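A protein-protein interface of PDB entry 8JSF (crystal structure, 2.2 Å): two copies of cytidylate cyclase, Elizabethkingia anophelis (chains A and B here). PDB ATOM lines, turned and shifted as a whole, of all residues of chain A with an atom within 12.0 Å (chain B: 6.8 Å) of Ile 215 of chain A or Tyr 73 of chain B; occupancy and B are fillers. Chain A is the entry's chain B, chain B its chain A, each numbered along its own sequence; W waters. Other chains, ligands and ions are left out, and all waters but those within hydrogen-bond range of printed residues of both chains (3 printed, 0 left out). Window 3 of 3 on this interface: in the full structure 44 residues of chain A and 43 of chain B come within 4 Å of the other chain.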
ATOM      1  N   GLY A  78       8.721  -4.161  26.225  1.00  0.00           N
ATOM      2  CA  GLY A  78       9.969  -3.430  26.360  1.00  0.00           C
ATOM      3  C   GLY A  78      10.711  -3.733  27.637  1.00  0.00           C
ATOM      4  O   GLY A  78      11.412  -2.863  28.165  1.00  0.00           O
ATOM      5  N   LEU A  86      17.723  -3.048  33.616  1.00  0.00           N
ATOM      6  CA  LEU A  86      18.536  -2.034  32.952  1.00  0.00           C
ATOM      7  C   LEU A  86      17.785  -0.727  32.730  1.00  0.00           C
ATOM      8  O   LEU A  86      18.411   0.267  32.348  1.00  0.00           O
ATOM      9  CB  LEU A  86      19.083  -2.569  31.625  1.00  0.00           C
ATOM     10  CG  LEU A  86      20.038  -3.755  31.775  1.00  0.00           C
ATOM     11  CD1 LEU A  86      20.316  -4.434  30.440  1.00  0.00           C
ATOM     12  CD2 LEU A  86      21.337  -3.284  32.419  1.00  0.00           C
ATOM     13  N   LYS A  87      16.472  -0.707  32.950  1.00  0.00           N
ATOM     14  CA  LYS A  87      15.705   0.522  32.797  1.00  0.00           C
ATOM     15  C   LYS A  87      16.190   1.571  33.789  1.00  0.00           C
ATOM     16  O   LYS A  87      16.562   1.245  34.918  1.00  0.00           O
ATOM     17  CB  LYS A  87      14.216   0.241  33.022  1.00  0.00           C
ATOM     18  CG  LYS A  87      13.314   1.478  32.990  1.00  0.00           C
ATOM     19  CD  LYS A  87      11.854   1.105  33.200  1.00  0.00           C
ATOM     20  CE  LYS A  87      10.961   2.337  33.161  1.00  0.00           C
ATOM     21  NZ  LYS A  87       9.542   2.013  33.464  1.00  0.00           N
ATOM     22  N   ASN A  88      16.198   2.834  33.352  1.00  0.00           N
ATOM     23  CA  ASN A  88      16.649   3.973  34.156  1.00  0.00           C
ATOM     24  C   ASN A  88      18.134   3.893  34.494  1.00  0.00           C
ATOM     25  O   ASN A  88      18.593   4.563  35.425  1.00  0.00           O
ATOM     26  CB  ASN A  88      15.837   4.118  35.452  1.00  0.00           C
ATOM     27  CG  ASN A  88      14.377   4.433  35.199  1.00  0.00           C
ATOM     28  OD1 ASN A  88      14.044   5.268  34.356  1.00  0.00           O
ATOM     29  ND2 ASN A  88      13.493   3.756  35.930  1.00  0.00           N
ATOM     30  N   THR A  89      18.907   3.084  33.771  1.00  0.00           N
ATOM     31  CA  THR A  89      20.334   2.970  34.030  1.00  0.00           C
ATOM     32  C   THR A  89      21.131   3.242  32.763  1.00  0.00           C
ATOM     33  O   THR A  89      20.602   3.275  31.649  1.00  0.00           O
ATOM     34  CB  THR A  89      20.724   1.578  34.558  1.00  0.00           C
ATOM     35  OG1 THR A  89      20.909   0.684  33.450  1.00  0.00           O
ATOM     36  CG2 THR A  89      19.662   1.022  35.486  1.00  0.00           C
ATOM     37  N   ASN A  90      22.435   3.415  32.966  1.00  0.00           N
ATOM     38  CA  ASN A  90      23.409   3.539  31.896  1.00  0.00           C
ATOM     39  C   ASN A  90      24.203   2.249  31.721  1.00  0.00           C
ATOM     40  O   ASN A  90      25.320   2.274  31.194  1.00  0.00           O
ATOM     41  CB  ASN A  90      24.346   4.713  32.197  1.00  0.00           C
ATOM     42  CG  ASN A  90      25.098   5.192  30.975  1.00  0.00           C
ATOM     43  OD1 ASN A  90      24.573   5.178  29.861  1.00  0.00           O
ATOM     44  ND2 ASN A  90      26.340   5.625  31.182  1.00  0.00           N
ATOM     45  N   HIS A 211      20.424  -3.113  26.568  1.00  0.00           N
ATOM     46  CA  HIS A 211      20.624  -1.796  27.152  1.00  0.00           C
ATOM     47  C   HIS A 211      19.294  -1.061  27.186  1.00  0.00           C
ATOM     48  O   HIS A 211      18.316  -1.459  26.544  1.00  0.00           O
ATOM     49  CB  HIS A 211      21.652  -0.995  26.350  1.00  0.00           C
ATOM     50  CG  HIS A 211      21.217  -0.709  24.945  1.00  0.00           C
ATOM     51  ND1 HIS A 211      20.428   0.372  24.619  1.00  0.00           N
ATOM     52  CD2 HIS A 211      21.450  -1.368  23.785  1.00  0.00           C
ATOM     53  CE1 HIS A 211      20.191   0.369  23.319  1.00  0.00           C
ATOM     54  NE2 HIS A 211      20.803  -0.676  22.789  1.00  0.00           N
ATOM     55  N   ASN A 212      19.296   0.065  27.893  1.00  0.00           N
ATOM     56  CA  ASN A 212      18.140   0.944  27.924  1.00  0.00           C
ATOM     57  C   ASN A 212      18.123   1.834  26.688  1.00  0.00           C
ATOM     58  O   ASN A 212      19.168   2.215  26.148  1.00  0.00           O
ATOM     59  CB  ASN A 212      18.142   1.806  29.189  1.00  0.00           C
ATOM     60  CG  ASN A 212      16.779   2.411  29.483  1.00  0.00           C
ATOM     61  OD1 ASN A 212      15.785   1.693  29.621  1.00  0.00           O
ATOM     62  ND2 ASN A 212      16.724   3.733  29.587  1.00  0.00           N
ATOM     63  N   ALA A 213      16.918   2.160  26.238  1.00  0.00           N
ATOM     64  CA  ALA A 213      16.707   3.053  25.113  1.00  0.00           C
ATOM     65  C   ALA A 213      15.600   4.013  25.501  1.00  0.00           C
ATOM     66  O   ALA A 213      14.631   3.617  26.158  1.00  0.00           O
ATOM     67  CB  ALA A 213      16.327   2.290  23.834  1.00  0.00           C
ATOM     68  N   GLY A 214      15.770   5.276  25.148  1.00  0.00           N
ATOM     69  CA  GLY A 214      14.792   6.270  25.496  1.00  0.00           C
ATOM     70  C   GLY A 214      15.178   6.950  26.787  1.00  0.00           C
ATOM     71  O   GLY A 214      16.333   6.931  27.216  1.00  0.00           O
ATOM     72  N   ILE A 215      14.186   7.573  27.412  1.00  0.00           N
ATOM     73  CA  ILE A 215      14.428   8.332  28.632  1.00  0.00           C
ATOM     74  C   ILE A 215      13.165   8.317  29.486  1.00  0.00           C
ATOM     75  O   ILE A 215      12.042   8.346  28.969  1.00  0.00           O
ATOM     76  CB  ILE A 215      14.918   9.760  28.307  1.00  0.00           C
ATOM     77  CG1 ILE A 215      15.383  10.468  29.583  1.00  0.00           C
ATOM     78  CG2 ILE A 215      13.850  10.543  27.561  1.00  0.00           C
ATOM     79  CD1 ILE A 215      16.414  11.553  29.336  1.00  0.00           C
ATOM     80  N   GLY A 216      13.361   8.251  30.803  1.00  0.00           N
ATOM     81  CA  GLY A 216      12.242   8.230  31.731  1.00  0.00           C
ATOM     82  C   GLY A 216      11.340   7.038  31.493  1.00  0.00           C
ATOM     83  O   GLY A 216      11.804   5.907  31.316  1.00  0.00           O
ATOM     84  N   GLU A 217      10.029   7.288  31.495  1.00  0.00           N
ATOM     85  CA  GLU A 217       9.058   6.250  31.172  1.00  0.00           C
ATOM     86  C   GLU A 217       8.925   6.046  29.669  1.00  0.00           C
ATOM     87  O   GLU A 217       8.364   5.033  29.239  1.00  0.00           O
ATOM     88  CB  GLU A 217       7.693   6.607  31.770  1.00  0.00           C
ATOM     89  CG  GLU A 217       7.651   6.584  33.302  1.00  0.00           C
ATOM     90  CD  GLU A 217       8.023   5.226  33.881  1.00  0.00           C
ATOM     91  OE1 GLU A 217       7.302   4.241  33.609  1.00  0.00           O
ATOM     92  OE2 GLU A 217       9.047   5.139  34.594  1.00  0.00           O
ATOM     93  N   CYS A 218       9.428   6.989  28.870  1.00  0.00           N
ATOM     94  CA  CYS A 218       9.452   6.865  27.413  1.00  0.00           C
ATOM     95  C   CYS A 218      10.685   6.052  27.027  1.00  0.00           C
ATOM     96  O   CYS A 218      11.657   6.549  26.456  1.00  0.00           O
ATOM     97  CB  CYS A 218       9.448   8.239  26.760  1.00  0.00           C
ATOM     98  SG  CYS A 218       9.447   8.216  24.959  1.00  0.00           S
ATOM     99  N   SER A 219      10.642   4.769  27.373  1.00  0.00           N
ATOM    100  CA  SER A 219      11.851   3.968  27.302  1.00  0.00           C
ATOM    101  C   SER A 219      11.496   2.499  27.161  1.00  0.00           C
ATOM    102  O   SER A 219      10.376   2.077  27.451  1.00  0.00           O
ATOM    103  CB  SER A 219      12.709   4.169  28.554  1.00  0.00           C
ATOM    104  OG  SER A 219      11.995   3.751  29.706  1.00  0.00           O
ATOM    105  N   GLU A 220      12.486   1.726  26.725  1.00  0.00           N
ATOM    106  CA  GLU A 220      12.378   0.276  26.713  1.00  0.00           C
ATOM    107  C   GLU A 220      13.767  -0.296  26.930  1.00  0.00           C
ATOM    108  O   GLU A 220      14.768   0.334  26.593  1.00  0.00           O
ATOM    109  CB  GLU A 220      11.783  -0.257  25.396  1.00  0.00           C
ATOM    110  CG  GLU A 220      12.602   0.057  24.151  1.00  0.00           C
ATOM    111  CD  GLU A 220      11.988  -0.511  22.871  1.00  0.00           C
ATOM    112  OE1 GLU A 220      10.805  -0.918  22.884  1.00  0.00           O
ATOM    113  OE2 GLU A 220      12.698  -0.552  21.847  1.00  0.00           O
ATOM    114  N   VAL A 221      13.829  -1.508  27.458  1.00  0.00           N
ATOM    115  CA  VAL A 221      15.072  -2.267  27.458  1.00  0.00           C
ATOM    116  C   VAL A 221      15.064  -3.145  26.217  1.00  0.00           C
ATOM    117  O   VAL A 221      14.114  -3.902  25.992  1.00  0.00           O
ATOM    118  CB  VAL A 221      15.228  -3.102  28.733  1.00  0.00           C
ATOM    119  CG1 VAL A 221      16.473  -3.957  28.633  1.00  0.00           C
ATOM    120  CG2 VAL A 221      15.286  -2.187  29.963  1.00  0.00           C
ATOM    121  N   THR A 222      16.104  -3.025  25.396  1.00  0.00           N
ATOM    122  CA  THR A 222      16.102  -3.654  24.086  1.00  0.00           C
ATOM    123  C   THR A 222      17.526  -4.071  23.742  1.00  0.00           C
ATOM    124  O   THR A 222      18.458  -3.886  24.532  1.00  0.00           O
ATOM    125  CB  THR A 222      15.510  -2.706  23.030  1.00  0.00           C
ATOM    126  OG1 THR A 222      15.293  -3.419  21.804  1.00  0.00           O
ATOM    127  CG2 THR A 222      16.449  -1.535  22.767  1.00  0.00           C
ATOM    128  N   THR B  71      10.318  18.564  28.478  1.00  0.00           N
ATOM    129  CA  THR B  71      10.426  17.122  28.629  1.00  0.00           C
ATOM    130  C   THR B  71       9.116  16.531  29.141  1.00  0.00           C
ATOM    131  O   THR B  71       8.321  17.199  29.806  1.00  0.00           O
ATOM    132  CB  THR B  71      11.571  16.756  29.577  1.00  0.00           C
ATOM    133  OG1 THR B  71      11.314  17.304  30.877  1.00  0.00           O
ATOM    134  CG2 THR B  71      12.883  17.316  29.048  1.00  0.00           C
ATOM    135  N   LYS B  72       8.911  15.247  28.832  1.00  0.00           N
ATOM    136  CA  LYS B  72       7.754  14.481  29.296  1.00  0.00           C
ATOM    137  C   LYS B  72       8.235  13.133  29.849  1.00  0.00           C
ATOM    138  O   LYS B  72       7.832  12.066  29.387  1.00  0.00           O
ATOM    139  CB  LYS B  72       6.767  14.270  28.147  1.00  0.00           C
ATOM    140  CG  LYS B  72       6.343  15.539  27.408  1.00  0.00           C
ATOM    141  CD  LYS B  72       5.514  16.456  28.279  1.00  0.00           C
ATOM    142  CE  LYS B  72       4.110  15.914  28.447  1.00  0.00           C
ATOM    143  NZ  LYS B  72       3.281  16.729  29.378  1.00  0.00           N
ATOM    144  N   TYR B  73       9.078  13.181  30.886  1.00  0.00           N
ATOM    145  CA  TYR B  73       9.709  11.965  31.400  1.00  0.00           C
ATOM    146  C   TYR B  73       8.735  10.973  32.029  1.00  0.00           C
ATOM    147  O   TYR B  73       9.103   9.808  32.209  1.00  0.00           O
ATOM    148  CB  TYR B  73      10.774  12.322  32.439  1.00  0.00           C
ATOM    149  CG  TYR B  73      11.941  13.108  31.896  1.00  0.00           C
ATOM    150  CD1 TYR B  73      12.505  12.794  30.672  1.00  0.00           C
ATOM    151  CD2 TYR B  73      12.472  14.177  32.609  1.00  0.00           C
ATOM    152  CE1 TYR B  73      13.571  13.515  30.173  1.00  0.00           C
ATOM    153  CE2 TYR B  73      13.537  14.904  32.118  1.00  0.00           C
ATOM    154  CZ  TYR B  73      14.083  14.566  30.898  1.00  0.00           C
ATOM    155  OH  TYR B  73      15.141  15.285  30.397  1.00  0.00           O
ATOM    156  N   GLU B  74       7.506  11.376  32.342  1.00  0.00           N
ATOM    157  CA  GLU B  74       6.574  10.474  33.005  1.00  0.00           C
ATOM    158  C   GLU B  74       5.550   9.857  32.063  1.00  0.00           C
ATOM    159  O   GLU B  74       4.724   9.057  32.513  1.00  0.00           O
ATOM    160  CB  GLU B  74       5.851  11.188  34.151  1.00  0.00           C
ATOM    161  CG  GLU B  74       6.782  11.855  35.147  1.00  0.00           C
ATOM    162  CD  GLU B  74       6.044  12.450  36.333  1.00  0.00           C
ATOM    163  OE1 GLU B  74       4.987  13.083  36.125  1.00  0.00           O
ATOM    164  OE2 GLU B  74       6.523  12.283  37.475  1.00  0.00           O
ATOM    165  N   GLU B  75       5.570  10.204  30.778  1.00  0.00           N
ATOM    166  CA  GLU B  75       4.631   9.613  29.831  1.00  0.00           C
ATOM    167  C   GLU B  75       5.150   8.249  29.390  1.00  0.00           C
ATOM    168  O   GLU B  75       6.155   8.151  28.678  1.00  0.00           O
ATOM    169  CB  GLU B  75       4.391  10.537  28.641  1.00  0.00           C
ATOM    170  CG  GLU B  75       3.542  11.741  29.004  1.00  0.00           C
ATOM    171  CD  GLU B  75       3.213  12.618  27.815  1.00  0.00           C
ATOM    172  OE1 GLU B  75       3.809  12.423  26.736  1.00  0.00           O
ATOM    173  OE2 GLU B  75       2.326  13.481  27.952  1.00  0.00           O
ATOM    174  N   LYS B  76       4.452   7.198  29.809  1.00  0.00           N
ATOM    175  CA  LYS B  76       4.770   5.846  29.392  1.00  0.00           C
ATOM    176  C   LYS B  76       4.408   5.642  27.923  1.00  0.00           C
ATOM    177  O   LYS B  76       3.653   6.414  27.324  1.00  0.00           O
ATOM    178  CB  LYS B  76       4.008   4.836  30.250  1.00  0.00           C
ATOM    179  CG  LYS B  76       4.259   4.972  31.738  1.00  0.00           C
ATOM    180  CD  LYS B  76       3.571   3.865  32.514  1.00  0.00           C
ATOM    181  CE  LYS B  76       3.678   4.096  34.015  1.00  0.00           C
ATOM    182  NZ  LYS B  76       2.750   3.207  34.775  1.00  0.00           N
ATOM    183  N   ARG B 124      20.708   5.475  19.726  1.00  0.00           N
ATOM    184  CA  ARG B 124      19.917   6.005  20.822  1.00  0.00           C
ATOM    185  C   ARG B 124      20.077   7.518  20.940  1.00  0.00           C
ATOM    186  O   ARG B 124      19.142   8.195  21.376  1.00  0.00           O
ATOM    187  CB  ARG B 124      20.241   5.232  22.107  1.00  0.00           C
ATOM    188  CG  ARG B 124      21.484   5.582  22.887  1.00  0.00           C
ATOM    189  CD  ARG B 124      21.514   4.714  24.159  1.00  0.00           C
ATOM    190  NE  ARG B 124      21.188   5.437  25.384  1.00  0.00           N
ATOM    191  CZ  ARG B 124      19.958   5.738  25.779  1.00  0.00           C
ATOM    192  NH1 ARG B 124      18.899   5.397  25.066  1.00  0.00           N
ATOM    193  NH2 ARG B 124      19.784   6.385  26.927  1.00  0.00           N
ATOM    194  N   LEU B 128      16.923   9.910  20.844  1.00  0.00           N
ATOM    195  CA  LEU B 128      16.665  10.933  21.855  1.00  0.00           C
ATOM    196  C   LEU B 128      16.404  12.285  21.205  1.00  0.00           C
ATOM    197  O   LEU B 128      15.519  13.033  21.639  1.00  0.00           O
ATOM    198  CB  LEU B 128      17.838  11.032  22.830  1.00  0.00           C
ATOM    199  CG  LEU B 128      17.989   9.920  23.867  1.00  0.00           C
ATOM    200  CD1 LEU B 128      19.295  10.076  24.621  1.00  0.00           C
ATOM    201  CD2 LEU B 128      16.807   9.914  24.831  1.00  0.00           C
ATOM    202  N   ILE B 131      12.865  12.129  19.967  1.00  0.00           N
ATOM    203  CA  ILE B 131      11.904  12.176  21.068  1.00  0.00           C
ATOM    204  C   ILE B 131      11.767  13.599  21.595  1.00  0.00           C
ATOM    205  O   ILE B 131      10.656  14.091  21.837  1.00  0.00           O
ATOM    206  CB  ILE B 131      12.332  11.208  22.187  1.00  0.00           C
ATOM    207  CG1 ILE B 131      12.219   9.753  21.717  1.00  0.00           C
ATOM    208  CG2 ILE B 131      11.525  11.462  23.454  1.00  0.00           C
ATOM    209  CD1 ILE B 131      12.807   8.747  22.697  1.00  0.00           C
ATOM    210  N   HIS B 132      12.896  14.276  21.798  1.00  0.00           N
ATOM    211  CA  HIS B 132      12.842  15.638  22.313  1.00  0.00           C
ATOM    212  C   HIS B 132      12.215  16.591  21.304  1.00  0.00           C
ATOM    213  O   HIS B 132      11.474  17.504  21.688  1.00  0.00           O
ATOM    214  CB  HIS B 132      14.236  16.096  22.726  1.00  0.00           C
ATOM    215  CG  HIS B 132      14.639  15.614  24.086  1.00  0.00           C
ATOM    216  ND1 HIS B 132      15.467  14.529  24.278  1.00  0.00           N
ATOM    217  CD2 HIS B 132      14.302  16.054  25.322  1.00  0.00           C
ATOM    218  CE1 HIS B 132      15.637  14.332  25.573  1.00  0.00           C
ATOM    219  NE2 HIS B 132      14.939  15.242  26.229  1.00  0.00           N
ATOM    220  N   TRP B 135       8.501  16.004  21.666  1.00  0.00           N
ATOM    221  CA  TRP B 135       8.031  16.593  22.917  1.00  0.00           C
ATOM    222  C   TRP B 135       7.927  18.107  22.813  1.00  0.00           C
ATOM    223  O   TRP B 135       6.976  18.709  23.324  1.00  0.00           O
ATOM    224  CB  TRP B 135       8.975  16.211  24.057  1.00  0.00           C
ATOM    225  CG  TRP B 135       8.755  14.840  24.603  1.00  0.00           C
ATOM    226  CD1 TRP B 135       7.709  14.005  24.338  1.00  0.00           C
ATOM    227  CD2 TRP B 135       9.628  14.125  25.484  1.00  0.00           C
ATOM    228  NE1 TRP B 135       7.863  12.821  25.022  1.00  0.00           N
ATOM    229  CE2 TRP B 135       9.038  12.868  25.727  1.00  0.00           C
ATOM    230  CE3 TRP B 135      10.847  14.428  26.097  1.00  0.00           C
ATOM    231  CZ2 TRP B 135       9.625  11.918  26.557  1.00  0.00           C
ATOM    232  CZ3 TRP B 135      11.430  13.481  26.920  1.00  0.00           C
ATOM    233  CH2 TRP B 135      10.817  12.242  27.144  1.00  0.00           C
ATOM    234  N   LEU B 144       8.395   2.931  20.650  1.00  0.00           N
ATOM    235  CA  LEU B 144       9.777   2.984  20.199  1.00  0.00           C
ATOM    236  C   LEU B 144      10.048   1.765  19.327  1.00  0.00           C
ATOM    237  O   LEU B 144       9.878   0.627  19.775  1.00  0.00           O
ATOM    238  CB  LEU B 144      10.754   3.005  21.377  1.00  0.00           C
ATOM    239  CG  LEU B 144      10.650   4.079  22.462  1.00  0.00           C
ATOM    240  CD1 LEU B 144      11.811   3.942  23.441  1.00  0.00           C
ATOM    241  CD2 LEU B 144      10.628   5.462  21.870  1.00  0.00           C
HETATM  242  O   HOH W   1      22.497   2.865  27.000  1.00  0.00           O
HETATM  243  O   HOH W   2      17.056   6.187  22.702  1.00  0.00           O
HETATM  244  O   HOH W   3       5.888   8.628  25.771  1.00  0.00           O
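Of chain B, only Tyr 73, Leu 128 and Trp 135 come within 4 Å of Ile 215 of chain A. Tyr 73 of chain B touches just these residues of chain A: Ile 215, Gly 216 and Glu 217. Lys 72 of chain B touches none of the printed residues of chain A. Of chain A, only Glu 217 comes within 4 Å of Glu 74 of chain B. Leu 128 of chain B touches just these residues of chain A: Gly 214 (3.8 Å) and Ile 215 (3.96 Å). No residue of chain A comes within 4 Å of Ile 131 of chain B. Printed residues of chain B within 4 Å of Ala 213 of chain A: Arg 124 (3.2 Å) and Leu 144 (3.9 Å). Printed residues of chain A within 4 Å of Trp 135 of chain B: Ile 215 and Cys 218. Of the printed residues of chain B, Glu 217 of chain A touches Tyr 73, Glu 74, Glu 75 and Lys 76. Of the printed residues of chain A, Arg 124 of chain B touches Asn 212, Ala 213 and Gly 214. Printed residues of chain B within 4 Å of Glu 220 of chain A: Leu 144 (3.6 Å). Asn 90 of chain A touches none of the printed residues of chain B. The nearest printed residue of chain B that does not touch Ala 213 of chain A is Leu 128 of chain B (6.1 Å).
Water W2 lies within hydrogen-bond range of the backbone NH of Gly 214 of chain A (2.9 Å) and the guanidinium group of Arg 124 of chain B (3.1 Å). Water W3 lies within hydrogen-bond range of the backbone carbonyl oxygen (O) of Glu 75 of chain B and the side-chain sulfur (SG) of Cys 218 of chain A. Water W1 bridges the guanidinium group (NE) of Arg 124 of chain B (3.3 Å) and the backbone carbonyl oxygen (O) of Asn 212 of chain A (3.5 Å).
Among the printed residues, pairs that only touch across the chains: Ala 213 of chain A with Arg 124 of chain B (3.2 Å), Ala 213 of chain A with Leu 144 of chain B (3.9 Å), Gly 214 of chain A with Leu 128 of chain B (3.8 Å), Ile 215 of chain A with Tyr 73 of chain B (3.6 Å), Ile 215 of chain A with Leu 128 of chain B (3.96 Å), Ile 215 of chain A with Trp 135 of chain B (3.5 Å), Gly 216 of chain A with Tyr 73 of chain B (3.5 Å), Glu 217 of chain A with Glu 74 of chain B (3.9 Å), Glu 217 of chain A with Glu 75 of chain B (3.6 Å), Glu 217 of chain A with Lys 76 of chain B (3.6 Å), Cys 218 of chain A with Trp 135 of chain B (3.7 Å), Cys 218 of chain A with Leu 144 of chain B (3.99 Å), Ser 219 of chain A with Leu 144 of chain B (3.9 Å) and Glu 220 of chain A with Leu 144 of chain B (3.6 Å).
The backbone NH (N) of Gly 214 of chain A lies close to the guanidinium group (NH1) of Arg 124 of chain B, at 3.1 Å. O of Glu 75 of chain B lies within hydrogen-bond range of N of Cys 218 of chain A, at 3.5 Å. O of Tyr 73 of chain B sits at hydrogen-bond distance from N of Glu 217 of chain A (2.8 Å). NH1 of Arg 124 of chain B is in hydrogen-bond range of O of Asn 212 of chain A, 3.4 Å away.
No position is printed for both chains. Of the 18 pairs that touch across the chains among the printed residues, none has its exchanged pair printed and touching as well.
OE1 of Glu 217 of chain A is in salt-bridge range of NZ of Lys 87 of chain A (3.2 Å). The backbone carbonyl oxygen of Glu 220 of chain A is in hydrogen-bond range of the backbone NH of Ala 213 of chain A, 2.8 Å away. The backbone carbonyl oxygen (O) of Gly 216 of chain A sits at hydrogen-bond distance from the side-chain hydroxyl (OG) of Ser 219 of chain A, at 2.7 Å. NZ of Lys 72 of chain B is in salt-bridge range of OE2 of Glu 75 of chain B, 3.7 Å away. The side-chain amide oxygen (OD1) of Asn 212 of chain A sits close to the backbone carbonyl oxygen (O) of Glu 220 of chain A (3.5 Å). O of Leu 128 of chain B sits at hydrogen-bond distance from ND1 of His 132 of chain B (3.0 Å).
Of the 18 printed residues of chain A, 9 touch a printed residue of chain B. Hydrophobic or aromatic side chains of chain A that line the printed part of chain B: Ile 215. Of the 12 printed residues of chain B, 8 touch a printed residue of chain A. Among the printed residues, 18 pairs touch across the chains. Among the printed residues, no Asp or Glu carboxylate lies within 4 Å of a Lys or Arg side-chain nitrogen of the other chain.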
